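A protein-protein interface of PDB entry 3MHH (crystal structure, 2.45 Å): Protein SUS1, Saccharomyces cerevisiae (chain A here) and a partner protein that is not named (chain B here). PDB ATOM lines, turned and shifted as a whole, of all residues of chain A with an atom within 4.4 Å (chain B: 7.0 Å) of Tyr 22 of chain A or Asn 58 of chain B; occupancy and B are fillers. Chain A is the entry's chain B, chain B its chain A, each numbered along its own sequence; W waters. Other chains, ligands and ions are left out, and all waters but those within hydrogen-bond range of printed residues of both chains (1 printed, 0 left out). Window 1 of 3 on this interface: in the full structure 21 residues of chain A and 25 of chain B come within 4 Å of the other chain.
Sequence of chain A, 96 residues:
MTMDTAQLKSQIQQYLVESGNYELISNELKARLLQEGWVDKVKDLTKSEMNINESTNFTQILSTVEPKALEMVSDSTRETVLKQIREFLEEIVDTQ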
ATOM      1  N   LEU A  16     -20.417   3.714  16.339  1.00  0.00           N
ATOM      2  CA  LEU A  16     -20.411   4.849  15.423  1.00  0.00           C
ATOM      3  C   LEU A  16     -21.294   4.535  14.232  1.00  0.00           C
ATOM      4  O   LEU A  16     -22.132   5.356  13.839  1.00  0.00           O
ATOM      5  CB  LEU A  16     -18.989   5.203  14.968  1.00  0.00           C
ATOM      6  CG  LEU A  16     -18.084   5.858  16.023  1.00  0.00           C
ATOM      7  CD1 LEU A  16     -16.665   6.118  15.482  1.00  0.00           C
ATOM      8  CD2 LEU A  16     -18.685   7.143  16.542  1.00  0.00           C
ATOM      9  N   VAL A  17     -21.126   3.337  13.677  1.00  0.00           N
ATOM     10  CA  VAL A  17     -21.935   2.914  12.533  1.00  0.00           C
ATOM     11  C   VAL A  17     -23.416   2.839  12.863  1.00  0.00           C
ATOM     12  O   VAL A  17     -24.243   3.391  12.144  1.00  0.00           O
ATOM     13  CB  VAL A  17     -21.477   1.557  11.984  1.00  0.00           C
ATOM     14  CG1 VAL A  17     -22.479   1.016  10.987  1.00  0.00           C
ATOM     15  CG2 VAL A  17     -20.070   1.680  11.337  1.00  0.00           C
ATOM     16  N   GLY A  20     -25.253   6.057  13.422  1.00  0.00           N
ATOM     17  CA  GLY A  20     -25.350   6.913  12.250  1.00  0.00           C
ATOM     18  C   GLY A  20     -24.199   7.901  12.132  1.00  0.00           C
ATOM     19  O   GLY A  20     -24.149   8.707  11.206  1.00  0.00           O
ATOM     20  N   ASN A  21     -23.252   7.833  13.054  1.00  0.00           N
ATOM     21  CA  ASN A  21     -22.198   8.829  13.089  1.00  0.00           C
ATOM     22  C   ASN A  21     -20.976   8.490  12.245  1.00  0.00           C
ATOM     23  O   ASN A  21     -20.215   9.389  11.870  1.00  0.00           O
ATOM     24  CB  ASN A  21     -21.837   9.156  14.538  1.00  0.00           C
ATOM     25  CG  ASN A  21     -22.988   9.830  15.258  1.00  0.00           C
ATOM     26  OD1 ASN A  21     -23.705  10.652  14.664  1.00  0.00           O
ATOM     27  ND2 ASN A  21     -23.212   9.461  16.509  1.00  0.00           N
ATOM     28  N   TYR A  22     -20.813   7.215  11.908  1.00  0.00           N
ATOM     29  CA  TYR A  22     -19.705   6.792  11.077  1.00  0.00           C
ATOM     30  C   TYR A  22     -19.928   7.305   9.655  1.00  0.00           C
ATOM     31  O   TYR A  22     -18.991   7.798   9.009  1.00  0.00           O
ATOM     32  CB  TYR A  22     -19.568   5.272  11.096  1.00  0.00           C
ATOM     33  CG  TYR A  22     -18.244   4.765  10.576  1.00  0.00           C
ATOM     34  CD1 TYR A  22     -17.135   4.669  11.405  1.00  0.00           C
ATOM     35  CD2 TYR A  22     -18.110   4.363   9.256  1.00  0.00           C
ATOM     36  CE1 TYR A  22     -15.918   4.198  10.923  1.00  0.00           C
ATOM     37  CE2 TYR A  22     -16.920   3.887   8.772  1.00  0.00           C
ATOM     38  CZ  TYR A  22     -15.821   3.810   9.597  1.00  0.00           C
ATOM     39  OH  TYR A  22     -14.638   3.332   9.082  1.00  0.00           O
ATOM     40  N   GLU A  23     -21.170   7.227   9.187  1.00  0.00           N
ATOM     41  CA  GLU A  23     -21.528   7.807   7.897  1.00  0.00           C
ATOM     42  C   GLU A  23     -21.139   9.272   7.850  1.00  0.00           C
ATOM     43  O   GLU A  23     -20.544   9.738   6.877  1.00  0.00           O
ATOM     44  CB  GLU A  23     -23.034   7.711   7.633  1.00  0.00           C
ATOM     45  CG  GLU A  23     -23.551   6.313   7.451  1.00  0.00           C
ATOM     46  CD  GLU A  23     -25.071   6.224   7.571  1.00  0.00           C
ATOM     47  OE1 GLU A  23     -25.763   6.581   6.578  1.00  0.00           O
ATOM     48  OE2 GLU A  23     -25.553   5.780   8.647  1.00  0.00           O
ATOM     49  N   LEU A  24     -21.511  10.015   8.884  1.00  0.00           N
ATOM     50  CA  LEU A  24     -21.290  11.453   8.875  1.00  0.00           C
ATOM     51  C   LEU A  24     -19.800  11.734   8.792  1.00  0.00           C
ATOM     52  O   LEU A  24     -19.364  12.583   8.020  1.00  0.00           O
ATOM     53  CB  LEU A  24     -21.913  12.103  10.107  1.00  0.00           C
ATOM     54  CG  LEU A  24     -23.436  11.918  10.207  1.00  0.00           C
ATOM     55  CD1 LEU A  24     -23.945  12.410  11.547  1.00  0.00           C
ATOM     56  CD2 LEU A  24     -24.180  12.628   9.068  1.00  0.00           C
ATOM     57  N   ILE A  25     -19.014  10.980   9.548  1.00  0.00           N
ATOM     58  CA  ILE A  25     -17.573  11.197   9.597  1.00  0.00           C
ATOM     59  C   ILE A  25     -16.955  10.835   8.259  1.00  0.00           C
ATOM     60  O   ILE A  25     -16.108  11.561   7.738  1.00  0.00           O
ATOM     61  CB  ILE A  25     -16.909  10.330  10.680  1.00  0.00           C
ATOM     62  CG1 ILE A  25     -17.507  10.632  12.050  1.00  0.00           C
ATOM     63  CG2 ILE A  25     -15.398  10.545  10.688  1.00  0.00           C
ATOM     64  CD1 ILE A  25     -17.363   9.487  13.020  1.00  0.00           C
ATOM     65  N   SER A  26     -17.351   9.683   7.728  1.00  0.00           N
ATOM     66  CA  SER A  26     -16.810   9.211   6.464  1.00  0.00           C
ATOM     67  C   SER A  26     -17.155  10.213   5.358  1.00  0.00           C
ATOM     68  O   SER A  26     -16.286  10.607   4.589  1.00  0.00           O
ATOM     69  CB  SER A  26     -17.361   7.817   6.130  1.00  0.00           C
ATOM     70  OG  SER A  26     -16.764   7.271   4.959  1.00  0.00           O
ATOM     71  N   PHE B  45     -21.511  -1.078   5.594  1.00  0.00           N
ATOM     72  CA  PHE B  45     -20.410  -1.054   6.559  1.00  0.00           C
ATOM     73  C   PHE B  45     -20.368  -2.311   7.398  1.00  0.00           C
ATOM     74  O   PHE B  45     -19.303  -2.931   7.548  1.00  0.00           O
ATOM     75  CB  PHE B  45     -20.501   0.149   7.504  1.00  0.00           C
ATOM     76  CG  PHE B  45     -20.052   1.448   6.882  1.00  0.00           C
ATOM     77  CD1 PHE B  45     -18.742   1.617   6.469  1.00  0.00           C
ATOM     78  CD2 PHE B  45     -20.943   2.510   6.738  1.00  0.00           C
ATOM     79  CE1 PHE B  45     -18.327   2.830   5.896  1.00  0.00           C
ATOM     80  CE2 PHE B  45     -20.538   3.715   6.197  1.00  0.00           C
ATOM     81  CZ  PHE B  45     -19.228   3.871   5.758  1.00  0.00           C
ATOM     82  N   THR B  48     -20.244  -5.738   4.671  1.00  0.00           N
ATOM     83  CA  THR B  48     -19.234  -5.925   3.620  1.00  0.00           C
ATOM     84  C   THR B  48     -17.901  -5.259   3.956  1.00  0.00           C
ATOM     85  O   THR B  48     -16.908  -5.463   3.254  1.00  0.00           O
ATOM     86  CB  THR B  48     -19.710  -5.396   2.245  1.00  0.00           C
ATOM     87  OG1 THR B  48     -19.679  -3.959   2.240  1.00  0.00           O
ATOM     88  CG2 THR B  48     -21.109  -5.891   1.942  1.00  0.00           C
ATOM     89  N   MET B  49     -17.876  -4.467   5.023  1.00  0.00           N
ATOM     90  CA  MET B  49     -16.662  -3.764   5.417  1.00  0.00           C
ATOM     91  C   MET B  49     -16.313  -4.038   6.858  1.00  0.00           C
ATOM     92  O   MET B  49     -15.614  -3.261   7.481  1.00  0.00           O
ATOM     93  CB  MET B  49     -16.819  -2.261   5.210  1.00  0.00           C
ATOM     94  CG  MET B  49     -16.784  -1.865   3.758  1.00  0.00           C
ATOM     95  SD  MET B  49     -17.437  -0.227   3.465  1.00  0.00           S
ATOM     96  CE  MET B  49     -17.355  -0.204   1.664  1.00  0.00           C
ATOM     97  N   LYS B  50     -16.791  -5.169   7.364  1.00  0.00           N
ATOM     98  CA  LYS B  50     -16.503  -5.608   8.718  1.00  0.00           C
ATOM     99  C   LYS B  50     -15.707  -6.895   8.591  1.00  0.00           C
ATOM    100  O   LYS B  50     -16.187  -7.873   8.025  1.00  0.00           O
ATOM    101  CB  LYS B  50     -17.814  -5.863   9.465  1.00  0.00           C
ATOM    102  CG  LYS B  50     -17.698  -6.620  10.795  1.00  0.00           C
ATOM    103  CD  LYS B  50     -17.794  -5.701  11.993  1.00  0.00           C
ATOM    104  CE  LYS B  50     -18.448  -6.400  13.185  1.00  0.00           C
ATOM    105  NZ  LYS B  50     -19.912  -6.589  12.989  1.00  0.00           N
ATOM    106  N   CYS B  51     -14.480  -6.885   9.092  1.00  0.00           N
ATOM    107  CA  CYS B  51     -13.613  -8.039   8.978  1.00  0.00           C
ATOM    108  C   CYS B  51     -14.079  -9.129   9.921  1.00  0.00           C
ATOM    109  O   CYS B  51     -14.297  -8.874  11.092  1.00  0.00           O
ATOM    110  CB  CYS B  51     -12.180  -7.637   9.320  1.00  0.00           C
ATOM    111  SG  CYS B  51     -10.977  -8.992   9.396  1.00  0.00           S
ATOM    112  N   GLU B  56     -13.073  -5.214  12.826  1.00  0.00           N
ATOM    113  CA  GLU B  56     -12.980  -3.774  12.557  1.00  0.00           C
ATOM    114  C   GLU B  56     -13.694  -3.353  11.268  1.00  0.00           C
ATOM    115  O   GLU B  56     -13.782  -4.099  10.288  1.00  0.00           O
ATOM    116  CB  GLU B  56     -11.523  -3.315  12.475  1.00  0.00           C
ATOM    117  CG  GLU B  56     -10.844  -3.109  13.820  1.00  0.00           C
ATOM    118  CD  GLU B  56      -9.377  -2.746  13.677  1.00  0.00           C
ATOM    119  OE1 GLU B  56      -8.520  -3.496  14.192  1.00  0.00           O
ATOM    120  OE2 GLU B  56      -9.077  -1.724  13.032  1.00  0.00           O
ATOM    121  N   ILE B  57     -14.194  -2.127  11.282  1.00  0.00           N
ATOM    122  CA  ILE B  57     -14.784  -1.559  10.113  1.00  0.00           C
ATOM    123  C   ILE B  57     -13.649  -0.908   9.362  1.00  0.00           C
ATOM    124  O   ILE B  57     -12.829  -0.218   9.962  1.00  0.00           O
ATOM    125  CB  ILE B  57     -15.824  -0.487  10.471  1.00  0.00           C
ATOM    126  CG1 ILE B  57     -16.819  -1.016  11.512  1.00  0.00           C
ATOM    127  CG2 ILE B  57     -16.546  -0.018   9.223  1.00  0.00           C
ATOM    128  CD1 ILE B  57     -17.598  -2.236  11.067  1.00  0.00           C
ATOM    129  N   ASN B  58     -13.577  -1.149   8.058  1.00  0.00           N
ATOM    130  CA  ASN B  58     -12.656  -0.405   7.213  1.00  0.00           C
ATOM    131  C   ASN B  58     -11.206  -0.531   7.631  1.00  0.00           C
ATOM    132  O   ASN B  58     -10.480   0.455   7.609  1.00  0.00           O
ATOM    133  CB  ASN B  58     -13.027   1.074   7.257  1.00  0.00           C
ATOM    134  CG  ASN B  58     -14.233   1.396   6.413  1.00  0.00           C
ATOM    135  OD1 ASN B  58     -14.915   2.400   6.631  1.00  0.00           O
ATOM    136  ND2 ASN B  58     -14.496   0.555   5.423  1.00  0.00           N
ATOM    137  N   SER B  59     -10.779  -1.719   8.047  1.00  0.00           N
ATOM    138  CA  SER B  59      -9.377  -1.915   8.407  1.00  0.00           C
ATOM    139  C   SER B  59      -8.589  -2.059   7.110  1.00  0.00           C
ATOM    140  O   SER B  59      -8.053  -3.117   6.820  1.00  0.00           O
ATOM    141  CB  SER B  59      -9.203  -3.154   9.301  1.00  0.00           C
ATOM    142  OG  SER B  59      -7.834  -3.445   9.518  1.00  0.00           O
ATOM    143  N   GLY B  60      -8.517  -0.968   6.349  1.00  0.00           N
ATOM    144  CA  GLY B  60      -8.138  -1.011   4.933  1.00  0.00           C
ATOM    145  C   GLY B  60      -9.296  -1.576   4.128  1.00  0.00           C
ATOM    146  O   GLY B  60     -10.393  -1.751   4.655  1.00  0.00           O
ATOM    147  N   ALA B  61      -9.062  -1.879   2.854  1.00  0.00           N
ATOM    148  CA  ALA B  61     -10.072  -2.538   2.048  1.00  0.00           C
ATOM    149  C   ALA B  61     -10.491  -3.823   2.734  1.00  0.00           C
ATOM    150  O   ALA B  61      -9.676  -4.493   3.372  1.00  0.00           O
ATOM    151  CB  ALA B  61      -9.534  -2.837   0.667  1.00  0.00           C
ATOM    152  N   THR B  62     -11.769  -4.154   2.618  1.00  0.00           N
ATOM    153  CA  THR B  62     -12.283  -5.409   3.136  1.00  0.00           C
ATOM    154  C   THR B  62     -12.706  -6.221   1.927  1.00  0.00           C
ATOM    155  O   THR B  62     -13.276  -5.673   0.991  1.00  0.00           O
ATOM    156  CB  THR B  62     -13.496  -5.178   4.055  1.00  0.00           C
ATOM    157  OG1 THR B  62     -13.179  -4.180   5.040  1.00  0.00           O
ATOM    158  CG2 THR B  62     -13.900  -6.460   4.731  1.00  0.00           C
ATOM    159  N   CYS B  73     -10.071  -8.289   6.144  1.00  0.00           N
ATOM    160  CA  CYS B  73      -9.452  -6.973   5.978  1.00  0.00           C
ATOM    161  C   CYS B  73      -8.038  -7.046   5.415  1.00  0.00           C
ATOM    162  O   CYS B  73      -7.393  -8.091   5.441  1.00  0.00           O
ATOM    163  CB  CYS B  73      -9.422  -6.222   7.314  1.00  0.00           C
ATOM    164  SG  CYS B  73      -8.116  -6.731   8.444  1.00  0.00           S
ATOM    165  N   ASN B  75      -5.478  -4.432   6.189  1.00  0.00           N
ATOM    166  CA  ASN B  75      -4.478  -3.847   7.073  1.00  0.00           C
ATOM    167  C   ASN B  75      -3.871  -4.815   8.082  1.00  0.00           C
ATOM    168  O   ASN B  75      -2.705  -4.672   8.450  1.00  0.00           O
ATOM    169  CB  ASN B  75      -5.052  -2.637   7.801  1.00  0.00           C
ATOM    170  CG  ASN B  75      -5.065  -1.410   6.947  1.00  0.00           C
ATOM    171  OD1 ASN B  75      -5.241  -0.306   7.447  1.00  0.00           O
ATOM    172  ND2 ASN B  75      -4.883  -1.588   5.643  1.00  0.00           N
ATOM    173  N   SER B  94     -14.901  -4.456  -1.222  1.00  0.00           N
ATOM    174  CA  SER B  94     -16.282  -3.987  -1.057  1.00  0.00           C
ATOM    175  C   SER B  94     -16.492  -2.479  -1.313  1.00  0.00           C
ATOM    176  O   SER B  94     -17.628  -2.019  -1.385  1.00  0.00           O
ATOM    177  CB  SER B  94     -16.837  -4.405   0.301  1.00  0.00           C
ATOM    178  OG  SER B  94     -16.049  -3.923   1.372  1.00  0.00           O
ATOM    179  N   ASN B  95     -15.403  -1.737  -1.509  1.00  0.00           N
ATOM    180  CA  ASN B  95     -15.466  -0.323  -1.924  1.00  0.00           C
ATOM    181  C   ASN B  95     -15.626  -0.128  -3.442  1.00  0.00           C
ATOM    182  O   ASN B  95     -15.998   0.954  -3.885  1.00  0.00           O
ATOM    183  CB  ASN B  95     -14.187   0.421  -1.512  1.00  0.00           C
ATOM    184  CG  ASN B  95     -14.117   0.692  -0.037  1.00  0.00           C
ATOM    185  OD1 ASN B  95     -14.805   1.590   0.471  1.00  0.00           O
ATOM    186  ND2 ASN B  95     -13.283  -0.085   0.677  1.00  0.00           N
HETATM  187  O   HOH W   1     -15.350   4.630   4.963  1.00  0.00           O
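OD1 of Asn 58 of chain B sits at hydrogen-bond distance from OH of Tyr 22 of chain A (2.6 Å).
O of Phe 45 of chain B is in hydrogen-bond range of N of Lys 50 of chain B (3.4 Å).
O of Met 49 of chain B sits at hydrogen-bond distance from N of Asn 58 of chain B (3.0 Å).
N of Tyr 22 of chain A sits at hydrogen-bond distance from O of Leu 16 of chain A.
Among the printed residues, pairs that only touch across the chains: Tyr 22 of chain A with Phe 45 of chain B and Tyr 22 of chain A with Ile 57 of chain B.
Printed residues of chain B within 4 Å of Tyr 22 of chain A: Phe 45 (3.4 Å), Ile 57 (3.9 Å) and Asn 58 (2.6 Å).
Printed residues of chain A within 4 Å of Phe 45 of chain B: Tyr 22 (3.4 Å).
Of the printed residues of chain A, Ile 57 of chain B touches Tyr 22 (3.9 Å).
Ser 59 of chain B touches none of the printed residues of chain A.
The nearest residue of chain B that does not touch Tyr 22 of chain A is Ser 59 of chain B (6.4 Å).
The nearest printed residue of chain A that does not touch Ile 57 of chain B is Val 17 of chain A (4.2 Å).
Of the 16 printed residues of chain B, 3 touch a printed residue of chain A.
Printed residues of chain B that touch a printed residue of chain A: Phe 45, Ile 57 and Asn 58.
Water W1 lies within hydrogen-bond range of OD1 of Asn 58 of chain B (2.8 Å) and OG of Ser 26 of chain A (3.0 Å).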
